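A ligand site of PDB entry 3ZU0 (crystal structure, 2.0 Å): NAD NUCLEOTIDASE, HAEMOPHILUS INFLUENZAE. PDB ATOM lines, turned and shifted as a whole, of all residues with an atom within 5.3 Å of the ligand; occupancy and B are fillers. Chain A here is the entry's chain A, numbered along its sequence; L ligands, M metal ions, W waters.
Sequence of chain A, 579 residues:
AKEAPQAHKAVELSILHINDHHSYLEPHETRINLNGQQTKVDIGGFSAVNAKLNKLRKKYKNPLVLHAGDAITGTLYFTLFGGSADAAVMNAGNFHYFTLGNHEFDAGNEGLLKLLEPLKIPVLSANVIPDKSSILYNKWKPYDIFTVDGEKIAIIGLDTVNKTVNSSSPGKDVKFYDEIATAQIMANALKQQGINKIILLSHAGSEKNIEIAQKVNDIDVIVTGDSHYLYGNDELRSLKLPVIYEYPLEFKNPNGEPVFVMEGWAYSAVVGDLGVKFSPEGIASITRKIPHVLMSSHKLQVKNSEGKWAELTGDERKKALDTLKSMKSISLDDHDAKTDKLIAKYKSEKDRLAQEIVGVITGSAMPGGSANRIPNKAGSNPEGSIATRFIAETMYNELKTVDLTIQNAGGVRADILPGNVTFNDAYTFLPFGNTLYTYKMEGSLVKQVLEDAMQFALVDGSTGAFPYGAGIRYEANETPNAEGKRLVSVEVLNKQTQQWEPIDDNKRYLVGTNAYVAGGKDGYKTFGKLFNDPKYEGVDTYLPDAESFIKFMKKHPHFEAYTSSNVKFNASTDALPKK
Residues that only touch the ligand: Tyr 516, Phe 432, Gly 410, Ser 167, Gly 411 and His 22. Hydrophobic or aromatic side chains that line the ligand: His 22, His 103, Phe 432 and Tyr 516. Of the 23 residues printed, 14 come within 4 Å of the ligand. The nearest printed residue that does not touch the ligand is Ala 465 (4.2 Å).
The side-chain hydroxyl of Ser 462 sits at hydrogen-bond distance from an oxygen (O8) of the ligand (2.9 Å). The guanidinium group (NH2) of Arg 413 lies within salt-bridge range of an oxygen (O4) of the ligand (2.8 Å). N5 of the ligand lies close to OD1 of Asn 408 (3.2 Å). A nitrogen (N4) of the ligand lies close to the side-chain amide oxygen of Asn 434 (2.8 Å). The backbone carbonyl oxygen (O) of Gly 464 sits at hydrogen-bond distance from an oxygen (O9) of the ligand (3.4 Å). O4 of the ligand is in salt-bridge range of NH2 of Arg 373 (2.9 Å). A ring nitrogen (NE2) of His 103 sits at hydrogen-bond distance from an oxygen (O3) of the ligand (3.5 Å). The side-chain carboxylate (OD2) of Asp 522 is in hydrogen-bond range of an oxygen (O9) of the ligand.
The side-chain amide nitrogen (ND2) of Asn 408 sits close to the side-chain amide nitrogen (ND2) of Asn 514 (3.0 Å). NH1 of Arg 413 sits at hydrogen-bond distance from O of Gly 410 (2.9 Å). The backbone carbonyl oxygen (O) of Gly 464 sits at hydrogen-bond distance from the backbone NH (N) of Gly 410. The side-chain carboxylate of Asp 522 lies within hydrogen-bond range of the side-chain hydroxyl of Ser 167 (3.0 Å). The side-chain carboxylate of Asp 522 lies close to the backbone NH of Ala 465 (3.4 Å). OD1 of Asn 408 lies within hydrogen-bond range of N of Gly 411, 3.3 Å away. A ring nitrogen (ND1) of His 103 sits at hydrogen-bond distance from the side-chain carboxylate of Asp 106 (2.7 Å). N of Gly 464 lies within hydrogen-bond range of OG of Ser 462, 2.9 Å away.
Water W1 lies within hydrogen-bond range of O of Asp 106 (2.7 Å), OG of Ser 169 (2.9 Å) and N2 of the ligand (2.9 Å).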
ATOM      1  N   HIS A  22       2.408  -1.222 -28.499  1.00  0.00           N
ATOM      2  CA  HIS A  22       3.136  -2.294 -27.848  1.00  0.00           C
ATOM      3  C   HIS A  22       2.391  -3.645 -27.838  1.00  0.00           C
ATOM      4  O   HIS A  22       2.345  -4.308 -26.813  1.00  0.00           O
ATOM      5  CB  HIS A  22       3.478  -1.898 -26.408  1.00  0.00           C
ATOM      6  CG  HIS A  22       4.655  -0.986 -26.289  1.00  0.00           C
ATOM      7  ND1 HIS A  22       5.957  -1.435 -26.350  1.00  0.00           N
ATOM      8  CD2 HIS A  22       4.726   0.359 -26.103  1.00  0.00           C
ATOM      9  CE1 HIS A  22       6.776  -0.409 -26.223  1.00  0.00           C
ATOM     10  NE2 HIS A  22       6.058   0.688 -26.061  1.00  0.00           N
ATOM     11  N   HIS A 103      11.754  -0.188 -29.317  1.00  0.00           N
ATOM     12  CA  HIS A 103      11.406  -1.604 -29.117  1.00  0.00           C
ATOM     13  C   HIS A 103      11.247  -2.411 -30.393  1.00  0.00           C
ATOM     14  O   HIS A 103      11.183  -3.619 -30.361  1.00  0.00           O
ATOM     15  CB  HIS A 103      10.189  -1.761 -28.198  1.00  0.00           C
ATOM     16  CG  HIS A 103      10.463  -1.307 -26.803  1.00  0.00           C
ATOM     17  ND1 HIS A 103      11.048  -2.120 -25.853  1.00  0.00           N
ATOM     18  CD2 HIS A 103      10.292  -0.103 -26.209  1.00  0.00           C
ATOM     19  CE1 HIS A 103      11.201  -1.446 -24.728  1.00  0.00           C
ATOM     20  NE2 HIS A 103      10.752  -0.218 -24.914  1.00  0.00           N
ATOM     21  N   ASP A 106      14.077  -4.924 -30.406  1.00  0.00           N
ATOM     22  CA  ASP A 106      14.230  -5.762 -29.211  1.00  0.00           C
ATOM     23  C   ASP A 106      14.583  -7.205 -29.548  1.00  0.00           C
ATOM     24  O   ASP A 106      15.193  -7.908 -28.750  1.00  0.00           O
ATOM     25  CB  ASP A 106      12.946  -5.741 -28.390  1.00  0.00           C
ATOM     26  CG  ASP A 106      12.914  -4.588 -27.402  1.00  0.00           C
ATOM     27  OD1 ASP A 106      13.788  -3.698 -27.509  1.00  0.00           O
ATOM     28  OD2 ASP A 106      12.022  -4.566 -26.523  1.00  0.00           O
ATOM     29  N   SER A 167      19.920  -0.257 -25.006  1.00  0.00           N
ATOM     30  CA  SER A 167      19.013  -1.178 -24.329  1.00  0.00           C
ATOM     31  C   SER A 167      18.130  -2.042 -25.228  1.00  0.00           C
ATOM     32  O   SER A 167      17.405  -2.903 -24.730  1.00  0.00           O
ATOM     33  CB  SER A 167      18.175  -0.422 -23.302  1.00  0.00           C
ATOM     34  OG  SER A 167      18.996   0.051 -22.233  1.00  0.00           O
ATOM     35  N   SER A 168      18.170  -1.806 -26.535  1.00  0.00           N
ATOM     36  CA  SER A 168      17.515  -2.713 -27.497  1.00  0.00           C
ATOM     37  C   SER A 168      18.636  -3.441 -28.230  1.00  0.00           C
ATOM     38  O   SER A 168      19.796  -3.305 -27.859  1.00  0.00           O
ATOM     39  CB  SER A 168      16.617  -1.928 -28.461  1.00  0.00           C
ATOM     40  OG  SER A 168      15.738  -2.779 -29.203  1.00  0.00           O
ATOM     41  N   SER A 169      18.311  -4.205 -29.266  1.00  0.00           N
ATOM     42  CA  SER A 169      19.318  -5.018 -29.964  1.00  0.00           C
ATOM     43  C   SER A 169      19.412  -4.822 -31.484  1.00  0.00           C
ATOM     44  O   SER A 169      19.367  -5.786 -32.238  1.00  0.00           O
ATOM     45  CB  SER A 169      19.058  -6.518 -29.690  1.00  0.00           C
ATOM     46  OG  SER A 169      19.130  -6.779 -28.314  1.00  0.00           O
ATOM     47  N   HIS A 228       5.005   7.822 -23.934  1.00  0.00           N
ATOM     48  CA  HIS A 228       3.755   7.277 -23.409  1.00  0.00           C
ATOM     49  C   HIS A 228       2.913   8.317 -22.645  1.00  0.00           C
ATOM     50  O   HIS A 228       2.061   7.931 -21.839  1.00  0.00           O
ATOM     51  CB  HIS A 228       4.005   6.062 -22.505  1.00  0.00           C
ATOM     52  CG  HIS A 228       4.616   4.883 -23.194  1.00  0.00           C
ATOM     53  ND1 HIS A 228       4.584   3.615 -22.657  1.00  0.00           N
ATOM     54  CD2 HIS A 228       5.293   4.776 -24.367  1.00  0.00           C
ATOM     55  CE1 HIS A 228       5.213   2.778 -23.467  1.00  0.00           C
ATOM     56  NE2 HIS A 228       5.646   3.454 -24.519  1.00  0.00           N
ATOM     57  N   TYR A 267      -0.546   2.074 -25.526  1.00  0.00           N
ATOM     58  CA  TYR A 267      -1.303   0.816 -25.375  1.00  0.00           C
ATOM     59  C   TYR A 267      -2.696   0.854 -26.034  1.00  0.00           C
ATOM     60  O   TYR A 267      -3.679   0.368 -25.467  1.00  0.00           O
ATOM     61  CB  TYR A 267      -1.410   0.438 -23.895  1.00  0.00           C
ATOM     62  CG  TYR A 267      -0.084   0.389 -23.162  1.00  0.00           C
ATOM     63  CD1 TYR A 267       1.082   0.012 -23.814  1.00  0.00           C
ATOM     64  CD2 TYR A 267       0.010   0.753 -21.829  1.00  0.00           C
ATOM     65  CE1 TYR A 267       2.310  -0.013 -23.156  1.00  0.00           C
ATOM     66  CE2 TYR A 267       1.230   0.742 -21.156  1.00  0.00           C
ATOM     67  CZ  TYR A 267       2.373   0.353 -21.827  1.00  0.00           C
ATOM     68  OH  TYR A 267       3.582   0.327 -21.177  1.00  0.00           O
ATOM     69  N   SER A 370       8.204  -4.147 -13.309  1.00  0.00           N
ATOM     70  CA  SER A 370       8.818  -2.831 -13.248  1.00  0.00           C
ATOM     71  C   SER A 370       8.885  -2.219 -11.864  1.00  0.00           C
ATOM     72  O   SER A 370       9.922  -1.691 -11.478  1.00  0.00           O
ATOM     73  CB  SER A 370       8.084  -1.862 -14.192  1.00  0.00           C
ATOM     74  OG  SER A 370       8.180  -2.313 -15.528  1.00  0.00           O
ATOM     75  N   ARG A 373      11.822  -3.520  -9.527  1.00  0.00           N
ATOM     76  CA  ARG A 373      13.172  -3.671 -10.059  1.00  0.00           C
ATOM     77  C   ARG A 373      14.268  -3.326  -9.056  1.00  0.00           C
ATOM     78  O   ARG A 373      15.278  -4.019  -8.979  1.00  0.00           O
ATOM     79  CB  ARG A 373      13.341  -2.834 -11.330  1.00  0.00           C
ATOM     80  CG  ARG A 373      12.627  -3.437 -12.531  1.00  0.00           C
ATOM     81  CD  ARG A 373      12.667  -2.495 -13.742  1.00  0.00           C
ATOM     82  NE  ARG A 373      12.081  -3.131 -14.909  1.00  0.00           N
ATOM     83  CZ  ARG A 373      12.057  -2.607 -16.135  1.00  0.00           C
ATOM     84  NH1 ARG A 373      12.579  -1.413 -16.347  1.00  0.00           N
ATOM     85  NH2 ARG A 373      11.494  -3.283 -17.135  1.00  0.00           N
ATOM     86  N   ASN A 408      19.404  -9.452 -15.275  1.00  0.00           N
ATOM     87  CA  ASN A 408      18.896  -8.106 -15.122  1.00  0.00           C
ATOM     88  C   ASN A 408      17.405  -8.122 -14.807  1.00  0.00           C
ATOM     89  O   ASN A 408      16.649  -8.898 -15.385  1.00  0.00           O
ATOM     90  CB  ASN A 408      19.183  -7.253 -16.365  1.00  0.00           C
ATOM     91  CG  ASN A 408      18.519  -7.790 -17.627  1.00  0.00           C
ATOM     92  OD1 ASN A 408      17.837  -7.044 -18.345  1.00  0.00           O
ATOM     93  ND2 ASN A 408      18.712  -9.065 -17.910  1.00  0.00           N
ATOM     94  N   GLY A 410      15.085  -6.121 -15.616  1.00  0.00           N
ATOM     95  CA  GLY A 410      14.248  -5.822 -16.770  1.00  0.00           C
ATOM     96  C   GLY A 410      13.998  -7.066 -17.619  1.00  0.00           C
ATOM     97  O   GLY A 410      13.104  -7.084 -18.450  1.00  0.00           O
ATOM     98  N   GLY A 411      14.805  -8.103 -17.404  1.00  0.00           N
ATOM     99  CA  GLY A 411      14.657  -9.331 -18.141  1.00  0.00           C
ATOM    100  C   GLY A 411      13.565 -10.237 -17.611  1.00  0.00           C
ATOM    101  O   GLY A 411      13.304 -11.299 -18.181  1.00  0.00           O
ATOM    102  N   ARG A 413       9.573 -10.001 -16.398  1.00  0.00           N
ATOM    103  CA  ARG A 413       8.521  -8.984 -16.655  1.00  0.00           C
ATOM    104  C   ARG A 413       7.284  -8.958 -15.745  1.00  0.00           C
ATOM    105  O   ARG A 413       6.400  -8.129 -15.956  1.00  0.00           O
ATOM    106  CB  ARG A 413       8.048  -9.075 -18.108  1.00  0.00           C
ATOM    107  CG  ARG A 413       9.194  -9.189 -19.128  1.00  0.00           C
ATOM    108  CD  ARG A 413      10.053  -7.920 -19.190  1.00  0.00           C
ATOM    109  NE  ARG A 413       9.272  -6.749 -19.585  1.00  0.00           N
ATOM    110  CZ  ARG A 413       9.775  -5.520 -19.734  1.00  0.00           C
ATOM    111  NH1 ARG A 413      11.083  -5.291 -19.543  1.00  0.00           N
ATOM    112  NH2 ARG A 413       8.984  -4.522 -20.079  1.00  0.00           N
ATOM    113  N   PHE A 432      11.970 -12.437 -24.289  1.00  0.00           N
ATOM    114  CA  PHE A 432      12.955 -11.858 -25.195  1.00  0.00           C
ATOM    115  C   PHE A 432      13.672 -12.854 -26.095  1.00  0.00           C
ATOM    116  O   PHE A 432      14.316 -12.455 -27.070  1.00  0.00           O
ATOM    117  CB  PHE A 432      13.980 -11.040 -24.411  1.00  0.00           C
ATOM    118  CG  PHE A 432      13.400  -9.796 -23.791  1.00  0.00           C
ATOM    119  CD1 PHE A 432      12.902  -8.783 -24.580  1.00  0.00           C
ATOM    120  CD2 PHE A 432      13.345  -9.657 -22.415  1.00  0.00           C
ATOM    121  CE1 PHE A 432      12.370  -7.636 -24.015  1.00  0.00           C
ATOM    122  CE2 PHE A 432      12.832  -8.511 -21.842  1.00  0.00           C
ATOM    123  CZ  PHE A 432      12.329  -7.499 -22.644  1.00  0.00           C
ATOM    124  N   ASN A 434      16.300 -14.695 -25.431  1.00  0.00           N
ATOM    125  CA  ASN A 434      17.738 -14.766 -25.251  1.00  0.00           C
ATOM    126  C   ASN A 434      18.164 -16.205 -25.103  1.00  0.00           C
ATOM    127  O   ASN A 434      17.392 -17.030 -24.647  1.00  0.00           O
ATOM    128  CB  ASN A 434      18.180 -14.062 -23.965  1.00  0.00           C
ATOM    129  CG  ASN A 434      17.805 -12.605 -23.913  1.00  0.00           C
ATOM    130  OD1 ASN A 434      17.347 -12.113 -22.868  1.00  0.00           O
ATOM    131  ND2 ASN A 434      17.977 -11.913 -25.044  1.00  0.00           N
ATOM    132  N   SER A 462      18.223   2.748 -17.789  1.00  0.00           N
ATOM    133  CA  SER A 462      17.002   2.046 -17.415  1.00  0.00           C
ATOM    134  C   SER A 462      17.085   1.255 -16.117  1.00  0.00           C
ATOM    135  O   SER A 462      18.066   0.552 -15.859  1.00  0.00           O
ATOM    136  CB  SER A 462      16.600   1.085 -18.541  1.00  0.00           C
ATOM    137  OG  SER A 462      15.624   0.142 -18.094  1.00  0.00           O
ATOM    138  N   THR A 463      16.012   1.335 -15.326  1.00  0.00           N
ATOM    139  CA  THR A 463      15.914   0.552 -14.114  1.00  0.00           C
ATOM    140  C   THR A 463      16.012  -0.951 -14.397  1.00  0.00           C
ATOM    141  O   THR A 463      16.366  -1.719 -13.521  1.00  0.00           O
ATOM    142  CB  THR A 463      14.618   0.861 -13.347  1.00  0.00           C
ATOM    143  OG1 THR A 463      13.489   0.614 -14.186  1.00  0.00           O
ATOM    144  CG2 THR A 463      14.599   2.330 -12.850  1.00  0.00           C
ATOM    145  N   GLY A 464      15.704  -1.367 -15.625  1.00  0.00           N
ATOM    146  CA  GLY A 464      15.740  -2.785 -15.968  1.00  0.00           C
ATOM    147  C   GLY A 464      17.132  -3.385 -15.838  1.00  0.00           C
ATOM    148  O   GLY A 464      17.286  -4.599 -15.895  1.00  0.00           O
ATOM    149  N   ALA A 465      18.143  -2.531 -15.668  1.00  0.00           N
ATOM    150  CA  ALA A 465      19.518  -3.015 -15.575  1.00  0.00           C
ATOM    151  C   ALA A 465      19.828  -3.629 -14.226  1.00  0.00           C
ATOM    152  O   ALA A 465      20.816  -4.326 -14.079  1.00  0.00           O
ATOM    153  CB  ALA A 465      20.499  -1.892 -15.848  1.00  0.00           C
ATOM    154  N   ASN A 514      22.431 -13.942 -19.366  1.00  0.00           N
ATOM    155  CA  ASN A 514      21.737 -14.030 -20.651  1.00  0.00           C
ATOM    156  C   ASN A 514      22.541 -13.311 -21.744  1.00  0.00           C
ATOM    157  O   ASN A 514      23.360 -12.434 -21.444  1.00  0.00           O
ATOM    158  CB  ASN A 514      20.305 -13.481 -20.550  1.00  0.00           C
ATOM    159  CG  ASN A 514      20.273 -11.993 -20.312  1.00  0.00           C
ATOM    160  OD1 ASN A 514      20.679 -11.211 -21.165  1.00  0.00           O
ATOM    161  ND2 ASN A 514      19.776 -11.576 -19.155  1.00  0.00           N
ATOM    162  N   TYR A 516      21.821 -11.084 -23.876  1.00  0.00           N
ATOM    163  CA  TYR A 516      21.604  -9.637 -23.952  1.00  0.00           C
ATOM    164  C   TYR A 516      22.642  -8.827 -23.148  1.00  0.00           C
ATOM    165  O   TYR A 516      23.429  -8.060 -23.729  1.00  0.00           O
ATOM    166  CB  TYR A 516      20.163  -9.324 -23.514  1.00  0.00           C
ATOM    167  CG  TYR A 516      19.771  -7.879 -23.331  1.00  0.00           C
ATOM    168  CD1 TYR A 516      19.462  -7.058 -24.426  1.00  0.00           C
ATOM    169  CD2 TYR A 516      19.626  -7.365 -22.056  1.00  0.00           C
ATOM    170  CE1 TYR A 516      19.065  -5.723 -24.229  1.00  0.00           C
ATOM    171  CE2 TYR A 516      19.241  -6.051 -21.861  1.00  0.00           C
ATOM    172  CZ  TYR A 516      18.967  -5.239 -22.936  1.00  0.00           C
ATOM    173  OH  TYR A 516      18.554  -3.947 -22.703  1.00  0.00           O
ATOM    174  N   ASP A 522      22.254  -2.636 -21.642  1.00  0.00           N
ATOM    175  CA  ASP A 522      21.737  -2.220 -20.347  1.00  0.00           C
ATOM    176  C   ASP A 522      22.902  -1.770 -19.451  1.00  0.00           C
ATOM    177  O   ASP A 522      22.846  -1.878 -18.229  1.00  0.00           O
ATOM    178  CB  ASP A 522      20.923  -3.359 -19.697  1.00  0.00           C
ATOM    179  CG  ASP A 522      19.469  -2.996 -19.470  1.00  0.00           C
ATOM    180  OD1 ASP A 522      18.998  -1.943 -19.962  1.00  0.00           O
ATOM    181  OD2 ASP A 522      18.771  -3.786 -18.819  1.00  0.00           O
HETATM  182  P1  LIG L   1       8.896  -1.009 -21.546  1.00  0.00           P
HETATM  183  O1  LIG L   1       7.999  -1.287 -20.289  1.00  0.00           O
HETATM  184  O2  LIG L   1       9.252  -2.360 -22.130  1.00  0.00           O
HETATM  185  O3  LIG L   1       8.172  -0.218 -22.554  1.00  0.00           O
HETATM  186  P2  LIG L   1      11.524  -1.098 -20.197  1.00  0.00           P
HETATM  187  O4  LIG L   1      10.795  -2.389 -19.797  1.00  0.00           O
HETATM  188  O5  LIG L   1      12.349  -0.382 -19.096  1.00  0.00           O
HETATM  189  C1  LIG L   1      10.342  -0.241 -21.074  1.00  0.00           C
HETATM  190  O6  LIG L   1      12.299  -1.578 -21.548  1.00  0.00           O
HETATM  191  C2  LIG L   1      13.688  -1.667 -21.523  1.00  0.00           C
HETATM  192  C3  LIG L   1      14.274  -2.668 -20.685  1.00  0.00           C
HETATM  193  O7  LIG L   1      13.903  -3.970 -21.225  1.00  0.00           O
HETATM  194  C4  LIG L   1      15.734  -2.718 -20.839  1.00  0.00           C
HETATM  195  O8  LIG L   1      16.405  -1.779 -20.104  1.00  0.00           O
HETATM  196  C5  LIG L   1      16.084  -4.107 -20.433  1.00  0.00           C
HETATM  197  O9  LIG L   1      16.238  -4.204 -19.071  1.00  0.00           O
HETATM  198  C6  LIG L   1      14.912  -4.887 -20.900  1.00  0.00           C
HETATM  199  N1  LIG L   1      15.266  -5.654 -22.071  1.00  0.00           N
HETATM  200  C7  LIG L   1      15.108  -5.265 -23.361  1.00  0.00           C
HETATM  201  N2  LIG L   1      15.573  -6.252 -24.120  1.00  0.00           N
HETATM  202  C8  LIG L   1      16.020  -7.289 -23.316  1.00  0.00           C
HETATM  203  C9  LIG L   1      16.591  -8.566 -23.558  1.00  0.00           C
HETATM  204  N3  LIG L   1      16.841  -9.061 -24.845  1.00  0.00           N
HETATM  205  N4  LIG L   1      16.892  -9.326 -22.517  1.00  0.00           N
HETATM  206  C10 LIG L   1      16.697  -8.906 -21.276  1.00  0.00           C
HETATM  207  N5  LIG L   1      16.164  -7.707 -20.996  1.00  0.00           N
HETATM  208  C11 LIG L   1      15.829  -6.897 -22.009  1.00  0.00           C
HETATM  209 ZN    ZN M   1       6.897   2.634 -25.983  1.00  0.00          ZN
HETATM  210  O   HOH W   1      16.660  -6.772 -26.810  1.00  0.00           O
